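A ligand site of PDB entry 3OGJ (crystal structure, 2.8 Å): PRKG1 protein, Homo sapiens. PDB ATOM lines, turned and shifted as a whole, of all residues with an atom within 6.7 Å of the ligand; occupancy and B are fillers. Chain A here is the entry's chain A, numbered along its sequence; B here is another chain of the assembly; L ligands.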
ATOM      1  N   ASN A  28       3.045 -20.899 -20.405  1.00  0.00           N
ATOM      2  CA  ASN A  28       2.553 -19.744 -19.660  1.00  0.00           C
ATOM      3  C   ASN A  28       3.466 -19.421 -18.491  1.00  0.00           C
ATOM      4  O   ASN A  28       3.817 -20.290 -17.700  1.00  0.00           O
ATOM      5  CB  ASN A  28       1.139 -19.954 -19.139  1.00  0.00           C
ATOM      6  CG  ASN A  28       0.690 -18.808 -18.284  1.00  0.00           C
ATOM      7  OD1 ASN A  28       0.865 -18.819 -17.072  1.00  0.00           O
ATOM      8  ND2 ASN A  28       0.121 -17.790 -18.921  1.00  0.00           N
ATOM      9  N   ILE A  58     -12.326 -11.517 -25.988  1.00  0.00           N
ATOM     10  CA  ILE A  58     -12.248 -10.898 -24.681  1.00  0.00           C
ATOM     11  C   ILE A  58     -12.193  -9.373 -24.805  1.00  0.00           C
ATOM     12  O   ILE A  58     -11.372  -8.842 -25.551  1.00  0.00           O
ATOM     13  CB  ILE A  58     -11.003 -11.380 -23.914  1.00  0.00           C
ATOM     14  CG1 ILE A  58     -11.274 -12.744 -23.280  1.00  0.00           C
ATOM     15  CG2 ILE A  58     -10.616 -10.387 -22.834  1.00  0.00           C
ATOM     16  CD1 ILE A  58     -10.168 -13.197 -22.360  1.00  0.00           C
ATOM     17  N   GLY A  64     -14.149 -11.469 -15.872  1.00  0.00           N
ATOM     18  CA  GLY A  64     -13.511 -12.663 -16.380  1.00  0.00           C
ATOM     19  C   GLY A  64     -14.233 -13.944 -16.000  1.00  0.00           C
ATOM     20  O   GLY A  64     -14.792 -14.052 -14.909  1.00  0.00           O
ATOM     21  N   LEU A  66     -13.435 -17.124 -18.409  1.00  0.00           N
ATOM     22  CA  LEU A  66     -12.759 -18.203 -19.126  1.00  0.00           C
ATOM     23  C   LEU A  66     -11.274 -17.957 -19.415  1.00  0.00           C
ATOM     24  O   LEU A  66     -10.885 -16.878 -19.856  1.00  0.00           O
ATOM     25  CB  LEU A  66     -13.476 -18.482 -20.450  1.00  0.00           C
ATOM     26  CG  LEU A  66     -14.963 -18.823 -20.415  1.00  0.00           C
ATOM     27  CD1 LEU A  66     -15.568 -18.648 -21.797  1.00  0.00           C
ATOM     28  CD2 LEU A  66     -15.202 -20.221 -19.901  1.00  0.00           C
ATOM     29  N   VAL A  77      -3.818  -8.896 -29.433  1.00  0.00           N
ATOM     30  CA  VAL A  77      -4.172  -8.342 -28.126  1.00  0.00           C
ATOM     31  C   VAL A  77      -3.969  -6.836 -28.097  1.00  0.00           C
ATOM     32  O   VAL A  77      -2.926  -6.341 -28.520  1.00  0.00           O
ATOM     33  CB  VAL A  77      -3.321  -8.978 -27.009  1.00  0.00           C
ATOM     34  CG1 VAL A  77      -3.723  -8.425 -25.659  1.00  0.00           C
ATOM     35  CG2 VAL A  77      -3.455 -10.480 -27.026  1.00  0.00           C
ATOM     36  N   THR A  78      -4.963  -6.094 -27.597  1.00  0.00           N
ATOM     37  CA  THR A  78      -4.876  -4.635 -27.530  1.00  0.00           C
ATOM     38  C   THR A  78      -5.347  -4.059 -26.196  1.00  0.00           C
ATOM     39  O   THR A  78      -5.830  -4.786 -25.329  1.00  0.00           O
ATOM     40  CB  THR A  78      -5.677  -3.956 -28.660  1.00  0.00           C
ATOM     41  OG1 THR A  78      -7.031  -3.749 -28.228  1.00  0.00           O
ATOM     42  CG2 THR A  78      -5.666  -4.796 -29.928  1.00  0.00           C
ATOM     43  N   LEU A  84      -0.691  -4.721 -28.414  1.00  0.00           N
ATOM     44  CA  LEU A  84       0.188  -5.270 -27.379  1.00  0.00           C
ATOM     45  C   LEU A  84       0.989  -6.482 -27.819  1.00  0.00           C
ATOM     46  O   LEU A  84       1.983  -6.831 -27.184  1.00  0.00           O
ATOM     47  CB  LEU A  84      -0.584  -5.575 -26.096  1.00  0.00           C
ATOM     48  CG  LEU A  84      -0.771  -4.405 -25.118  1.00  0.00           C
ATOM     49  CD1 LEU A  84      -1.957  -3.548 -25.523  1.00  0.00           C
ATOM     50  CD2 LEU A  84      -0.944  -4.908 -23.695  1.00  0.00           C
ATOM     51  N   CYS A  85       0.549  -7.131 -28.893  1.00  0.00           N
ATOM     52  CA  CYS A  85       1.273  -8.242 -29.517  1.00  0.00           C
ATOM     53  C   CYS A  85       0.360  -9.137 -30.342  1.00  0.00           C
ATOM     54  O   CYS A  85      -0.793  -9.365 -29.976  1.00  0.00           O
ATOM     55  CB  CYS A  85       1.997  -9.102 -28.465  1.00  0.00           C
ATOM     56  SG  CYS A  85       0.965 -10.338 -27.645  1.00  0.00           S
ATOM     57  N   MET A  87      -0.425 -12.992 -31.766  1.00  0.00           N
ATOM     58  CA  MET A  87      -0.491 -14.209 -30.953  1.00  0.00           C
ATOM     59  C   MET A  87      -1.045 -15.375 -31.757  1.00  0.00           C
ATOM     60  O   MET A  87      -2.009 -15.222 -32.492  1.00  0.00           O
ATOM     61  CB  MET A  87      -1.363 -13.959 -29.716  1.00  0.00           C
ATOM     62  CG  MET A  87      -1.324 -15.052 -28.665  1.00  0.00           C
ATOM     63  SD  MET A  87      -2.167 -14.583 -27.132  1.00  0.00           S
ATOM     64  CE  MET A  87      -0.980 -13.464 -26.398  1.00  0.00           C
ATOM     65  N   VAL A  92      -1.266 -19.374 -24.154  1.00  0.00           N
ATOM     66  CA  VAL A  92      -2.366 -19.247 -23.205  1.00  0.00           C
ATOM     67  C   VAL A  92      -2.695 -17.774 -23.017  1.00  0.00           C
ATOM     68  O   VAL A  92      -1.790 -16.952 -22.851  1.00  0.00           O
ATOM     69  CB  VAL A  92      -2.004 -19.843 -21.847  1.00  0.00           C
ATOM     70  CG1 VAL A  92      -3.088 -19.516 -20.827  1.00  0.00           C
ATOM     71  CG2 VAL A  92      -1.807 -21.337 -21.967  1.00  0.00           C
ATOM     72  N   PHE A  93      -3.971 -17.443 -23.044  1.00  0.00           N
ATOM     73  CA  PHE A  93      -4.392 -16.071 -22.753  1.00  0.00           C
ATOM     74  C   PHE A  93      -5.678 -16.032 -21.939  1.00  0.00           C
ATOM     75  O   PHE A  93      -6.482 -16.961 -21.997  1.00  0.00           O
ATOM     76  CB  PHE A  93      -4.537 -15.253 -24.038  1.00  0.00           C
ATOM     77  CG  PHE A  93      -5.712 -15.657 -24.877  1.00  0.00           C
ATOM     78  CD1 PHE A  93      -5.530 -16.274 -26.101  1.00  0.00           C
ATOM     79  CD2 PHE A  93      -7.008 -15.398 -24.450  1.00  0.00           C
ATOM     80  CE1 PHE A  93      -6.616 -16.637 -26.887  1.00  0.00           C
ATOM     81  CE2 PHE A  93      -8.094 -15.761 -25.236  1.00  0.00           C
ATOM     82  CZ  PHE A  93      -7.893 -16.383 -26.450  1.00  0.00           C
ATOM     83  N   GLY A  94      -5.861 -14.945 -21.194  1.00  0.00           N
ATOM     84  CA  GLY A  94      -7.055 -14.752 -20.382  1.00  0.00           C
ATOM     85  C   GLY A  94      -6.862 -15.327 -18.992  1.00  0.00           C
ATOM     86  O   GLY A  94      -7.817 -15.665 -18.310  1.00  0.00           O
ATOM     87  N   GLU A  95      -5.605 -15.432 -18.570  1.00  0.00           N
ATOM     88  CA  GLU A  95      -5.287 -15.983 -17.270  1.00  0.00           C
ATOM     89  C   GLU A  95      -5.282 -14.896 -16.194  1.00  0.00           C
ATOM     90  O   GLU A  95      -5.552 -15.145 -15.020  1.00  0.00           O
ATOM     91  CB  GLU A  95      -3.925 -16.696 -17.309  1.00  0.00           C
ATOM     92  CG  GLU A  95      -2.682 -15.781 -17.383  1.00  0.00           C
ATOM     93  CD  GLU A  95      -2.357 -15.298 -18.790  1.00  0.00           C
ATOM     94  OE1 GLU A  95      -3.229 -15.419 -19.673  1.00  0.00           O
ATOM     95  OE2 GLU A  95      -1.227 -14.799 -19.002  1.00  0.00           O
ATOM     96  N   LEU A  96      -4.997 -13.666 -16.613  1.00  0.00           N
ATOM     97  CA  LEU A  96      -4.784 -12.571 -15.691  1.00  0.00           C
ATOM     98  C   LEU A  96      -6.021 -12.225 -14.861  1.00  0.00           C
ATOM     99  O   LEU A  96      -5.937 -12.115 -13.635  1.00  0.00           O
ATOM    100  CB  LEU A  96      -4.300 -11.337 -16.454  1.00  0.00           C
ATOM    101  CG  LEU A  96      -2.998 -11.585 -17.230  1.00  0.00           C
ATOM    102  CD1 LEU A  96      -2.394 -10.274 -17.702  1.00  0.00           C
ATOM    103  CD2 LEU A  96      -2.024 -12.368 -16.365  1.00  0.00           C
ATOM    104  N   ALA A  97      -7.172 -12.078 -15.512  1.00  0.00           N
ATOM    105  CA  ALA A  97      -8.397 -11.740 -14.810  1.00  0.00           C
ATOM    106  C   ALA A  97      -8.777 -12.784 -13.762  1.00  0.00           C
ATOM    107  O   ALA A  97      -9.374 -12.454 -12.744  1.00  0.00           O
ATOM    108  CB  ALA A  97      -9.539 -11.547 -15.772  1.00  0.00           C
ATOM    109  N   ILE A  98      -8.431 -14.036 -14.013  1.00  0.00           N
ATOM    110  CA  ILE A  98      -8.725 -15.100 -13.055  1.00  0.00           C
ATOM    111  C   ILE A  98      -7.719 -15.065 -11.908  1.00  0.00           C
ATOM    112  O   ILE A  98      -8.093 -15.124 -10.734  1.00  0.00           O
ATOM    113  CB  ILE A  98      -8.680 -16.504 -13.698  1.00  0.00           C
ATOM    114  CG1 ILE A  98      -9.963 -16.789 -14.488  1.00  0.00           C
ATOM    115  CG2 ILE A  98      -8.513 -17.569 -12.637  1.00  0.00           C
ATOM    116  CD1 ILE A  98     -10.245 -15.805 -15.622  1.00  0.00           C
ATOM    117  N   CYS A 102     -10.034  -9.916 -10.792  1.00  0.00           N
ATOM    118  CA  CYS A 102     -10.283  -8.584 -11.338  1.00  0.00           C
ATOM    119  C   CYS A 102     -10.946  -8.652 -12.703  1.00  0.00           C
ATOM    120  O   CYS A 102     -11.575  -9.655 -13.052  1.00  0.00           O
ATOM    121  CB  CYS A 102      -8.982  -7.782 -11.411  1.00  0.00           C
ATOM    122  SG  CYS A 102      -7.875  -8.245 -12.760  1.00  0.00           S
ATOM    123  N   THR A 103     -10.814  -7.592 -13.485  1.00  0.00           N
ATOM    124  CA  THR A 103     -11.420  -7.544 -14.808  1.00  0.00           C
ATOM    125  C   THR A 103     -10.407  -7.762 -15.932  1.00  0.00           C
ATOM    126  O   THR A 103      -9.214  -7.529 -15.746  1.00  0.00           O
ATOM    127  CB  THR A 103     -12.143  -6.214 -15.066  1.00  0.00           C
ATOM    128  OG1 THR A 103     -11.193  -5.146 -15.028  1.00  0.00           O
ATOM    129  CG2 THR A 103     -13.217  -5.981 -14.014  1.00  0.00           C
ATOM    130  N   ARG A 104     -10.909  -8.197 -17.083  1.00  0.00           N
ATOM    131  CA  ARG A 104     -10.063  -8.359 -18.260  1.00  0.00           C
ATOM    132  C   ARG A 104      -9.222  -7.116 -18.430  1.00  0.00           C
ATOM    133  O   ARG A 104      -9.711  -5.994 -18.240  1.00  0.00           O
ATOM    134  CB  ARG A 104     -10.917  -8.588 -19.515  1.00  0.00           C
ATOM    135  CG  ARG A 104     -11.778  -9.846 -19.469  1.00  0.00           C
ATOM    136  CD  ARG A 104     -10.927 -11.096 -19.399  1.00  0.00           C
ATOM    137  NE  ARG A 104     -11.755 -12.305 -19.326  1.00  0.00           N
ATOM    138  CZ  ARG A 104     -11.282 -13.545 -19.244  1.00  0.00           C
ATOM    139  NH1 ARG A 104      -9.973 -13.760 -19.217  1.00  0.00           N
ATOM    140  NH2 ARG A 104     -12.121 -14.563 -19.184  1.00  0.00           N
ATOM    141  N   THR A 105      -7.962  -7.307 -18.787  1.00  0.00           N
ATOM    142  CA  THR A 105      -7.012  -6.197 -18.879  1.00  0.00           C
ATOM    143  C   THR A 105      -6.629  -5.899 -20.325  1.00  0.00           C
ATOM    144  O   THR A 105      -5.757  -5.072 -20.580  1.00  0.00           O
ATOM    145  CB  THR A 105      -5.752  -6.480 -18.041  1.00  0.00           C
ATOM    146  OG1 THR A 105      -4.811  -7.211 -18.836  1.00  0.00           O
ATOM    147  CG2 THR A 105      -6.109  -7.287 -16.796  1.00  0.00           C
ATOM    148  N   ALA A 106      -7.272  -6.575 -21.271  1.00  0.00           N
ATOM    149  CA  ALA A 106      -6.980  -6.367 -22.681  1.00  0.00           C
ATOM    150  C   ALA A 106      -8.121  -6.845 -23.581  1.00  0.00           C
ATOM    151  O   ALA A 106      -9.048  -7.521 -23.114  1.00  0.00           O
ATOM    152  CB  ALA A 106      -5.685  -7.069 -23.054  1.00  0.00           C
ATOM    153  N   THR A 107      -8.035  -6.489 -24.849  1.00  0.00           N
ATOM    154  CA  THR A 107      -9.046  -6.843 -25.841  1.00  0.00           C
ATOM    155  C   THR A 107      -8.483  -7.732 -26.931  1.00  0.00           C
ATOM    156  O   THR A 107      -7.610  -7.325 -27.697  1.00  0.00           O
ATOM    157  CB  THR A 107      -9.669  -5.592 -26.490  1.00  0.00           C
ATOM    158  OG1 THR A 107     -10.323  -4.793 -25.489  1.00  0.00           O
ATOM    159  CG2 THR A 107     -10.687  -5.986 -27.550  1.00  0.00           C
ATOM    160  N   VAL A 108      -8.981  -8.968 -26.999  1.00  0.00           N
ATOM    161  CA  VAL A 108      -8.494  -9.946 -27.964  1.00  0.00           C
ATOM    162  C   VAL A 108      -9.423 -10.089 -29.166  1.00  0.00           C
ATOM    163  O   VAL A 108     -10.608 -10.371 -29.015  1.00  0.00           O
ATOM    164  CB  VAL A 108      -8.320 -11.327 -27.314  1.00  0.00           C
ATOM    165  CG1 VAL A 108      -7.604 -12.259 -28.267  1.00  0.00           C
ATOM    166  CG2 VAL A 108      -7.557 -11.223 -26.010  1.00  0.00           C
ATOM    167  N   LYS B  79       2.015  -5.570 -14.456  1.00  0.00           N
ATOM    168  CA  LYS B  79       2.860  -6.612 -15.040  1.00  0.00           C
ATOM    169  C   LYS B  79       3.433  -6.105 -16.364  1.00  0.00           C
ATOM    170  O   LYS B  79       2.692  -5.777 -17.293  1.00  0.00           O
ATOM    171  CB  LYS B  79       2.084  -7.912 -15.249  1.00  0.00           C
ATOM    172  CG  LYS B  79       2.956  -9.098 -15.637  1.00  0.00           C
ATOM    173  CD  LYS B  79       2.224 -10.419 -15.485  1.00  0.00           C
ATOM    174  CE  LYS B  79       3.202 -11.596 -15.594  1.00  0.00           C
ATOM    175  NZ  LYS B  79       2.535 -12.926 -15.465  1.00  0.00           N
ATOM    176  N   GLU B  80       4.753  -6.044 -16.447  1.00  0.00           N
ATOM    177  CA  GLU B  80       5.419  -5.507 -17.614  1.00  0.00           C
ATOM    178  C   GLU B  80       4.909  -4.095 -17.899  1.00  0.00           C
ATOM    179  O   GLU B  80       4.476  -3.803 -19.015  1.00  0.00           O
ATOM    180  CB  GLU B  80       5.182  -6.398 -18.837  1.00  0.00           C
ATOM    181  CG  GLU B  80       5.772  -7.795 -18.730  1.00  0.00           C
ATOM    182  CD  GLU B  80       5.438  -8.656 -19.932  1.00  0.00           C
ATOM    183  OE1 GLU B  80       4.482  -8.316 -20.668  1.00  0.00           O
ATOM    184  OE2 GLU B  80       6.129  -9.675 -20.147  1.00  0.00           O
ATOM    185  N   VAL B  82       2.276  -2.682 -17.336  1.00  0.00           N
ATOM    186  CA  VAL B  82       0.861  -2.598 -17.717  1.00  0.00           C
ATOM    187  C   VAL B  82      -0.035  -2.585 -16.480  1.00  0.00           C
ATOM    188  O   VAL B  82       0.018  -3.494 -15.654  1.00  0.00           O
ATOM    189  CB  VAL B  82       0.458  -3.776 -18.623  1.00  0.00           C
ATOM    190  CG1 VAL B  82      -1.001  -3.627 -19.073  1.00  0.00           C
ATOM    191  CG2 VAL B  82       1.384  -3.868 -19.827  1.00  0.00           C
ATOM    192  N   LEU B  84      -2.818  -3.442 -14.374  1.00  0.00           N
ATOM    193  CA  LEU B  84      -3.834  -4.491 -14.333  1.00  0.00           C
ATOM    194  C   LEU B  84      -5.075  -4.044 -13.579  1.00  0.00           C
ATOM    195  O   LEU B  84      -6.171  -3.989 -14.154  1.00  0.00           O
ATOM    196  CB  LEU B  84      -3.252  -5.756 -13.674  1.00  0.00           C
ATOM    197  CG  LEU B  84      -1.909  -6.211 -14.248  1.00  0.00           C
ATOM    198  CD1 LEU B  84      -1.421  -7.453 -13.522  1.00  0.00           C
ATOM    199  CD2 LEU B  84      -2.012  -6.447 -15.740  1.00  0.00           C
HETATM  200  P1  LIG L   1      -6.786 -11.185 -19.227  1.00  0.00           P
HETATM  201  O1  LIG L   1      -6.341  -9.959 -18.467  1.00  0.00           O
HETATM  202  O2  LIG L   1      -7.772 -11.946 -18.370  1.00  0.00           O
HETATM  203  O3  LIG L   1      -7.444 -10.724 -20.644  1.00  0.00           O
HETATM  204  C1  LIG L   1      -6.660 -10.363 -21.775  1.00  0.00           C
HETATM  205  C2  LIG L   1      -5.521 -11.328 -21.898  1.00  0.00           C
HETATM  206  O4  LIG L   1      -4.533 -10.918 -22.870  1.00  0.00           O
HETATM  207  C3  LIG L   1      -4.710 -11.428 -20.624  1.00  0.00           C
HETATM  208  O5  LIG L   1      -5.483 -12.058 -19.635  1.00  0.00           O
HETATM  209  C4  LIG L   1      -3.447 -12.116 -21.114  1.00  0.00           C
HETATM  210  O6  LIG L   1      -3.683 -13.489 -21.361  1.00  0.00           O
HETATM  211  C5  LIG L   1      -3.260 -11.396 -22.455  1.00  0.00           C
HETATM  212  N1  LIG L   1      -2.380 -10.224 -22.337  1.00  0.00           N
HETATM  213  C6  LIG L   1      -2.634  -9.114 -21.609  1.00  0.00           C
HETATM  214  N2  LIG L   1      -1.629  -8.212 -21.707  1.00  0.00           N
HETATM  215  C7  LIG L   1      -0.698  -8.746 -22.523  1.00  0.00           C
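N of Leu 96 is in hydrogen-bond range of O5 of the ligand. N of Ala 97 is in hydrogen-bond range of O2 of the ligand (2.9 Å). The backbone NH (N) of Gly 94 is in hydrogen-bond range of an oxygen (O6) of the ligand, at 2.6 Å. NH1 of Arg 104 is in salt-bridge range of O2 of the ligand (3.0 Å). The side-chain hydroxyl of Thr 105 sits close to an oxygen (O1) of the ligand, at 3.2 Å. An oxygen (O6) of the ligand sits at hydrogen-bond distance from the side-chain carboxylate (OE1) of Glu 95, 2.6 Å away. The backbone NH (N) of Thr 105 lies within hydrogen-bond range of an oxygen (O1) of the ligand, 3.1 Å away.
The guanidinium group (NH1) of Arg 104 is in hydrogen-bond range of the backbone carbonyl oxygen (O) of Gly 94, 3.0 Å away. The side-chain carboxylate (OE2) of Glu 95 sits at hydrogen-bond distance from the side-chain amide nitrogen (ND2) of Asn 28. N of Val 77 is in hydrogen-bond range of O of Cys 85, at 3.1 Å. The backbone carbonyl oxygen of Ile 58 sits at hydrogen-bond distance from the backbone NH of Val 108 (2.8 Å). O of Leu 66 is in hydrogen-bond range of NH2 of Arg 104, at 2.7 Å. O of Val 77 sits at hydrogen-bond distance from N of Leu 84 of chain A, 2.8 Å away. The backbone carbonyl oxygen of Ala 97 sits at hydrogen-bond distance from the backbone NH of Cys 102, at 3.3 Å.
Ile 58 touches the ligand (CG2 to O3, 3.9 Å). Val 77 touches the ligand (CG1 to O4, 3.8 Å). Leu 84 of chain A touches the ligand. CA of Phe 93 touches O6 of the ligand (3.0 Å). Ala 106 touches the ligand (CB to C1, 3.7 Å). Hydrophobic or aromatic side chains within 4 Å of the ligand: Ile 58, Val 77, Leu 84 of chain A, Phe 93, Leu 96, Ala 97 and Ala 106. Along chain A the residues within 4 Å of the ligand span positions 58 to 106.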
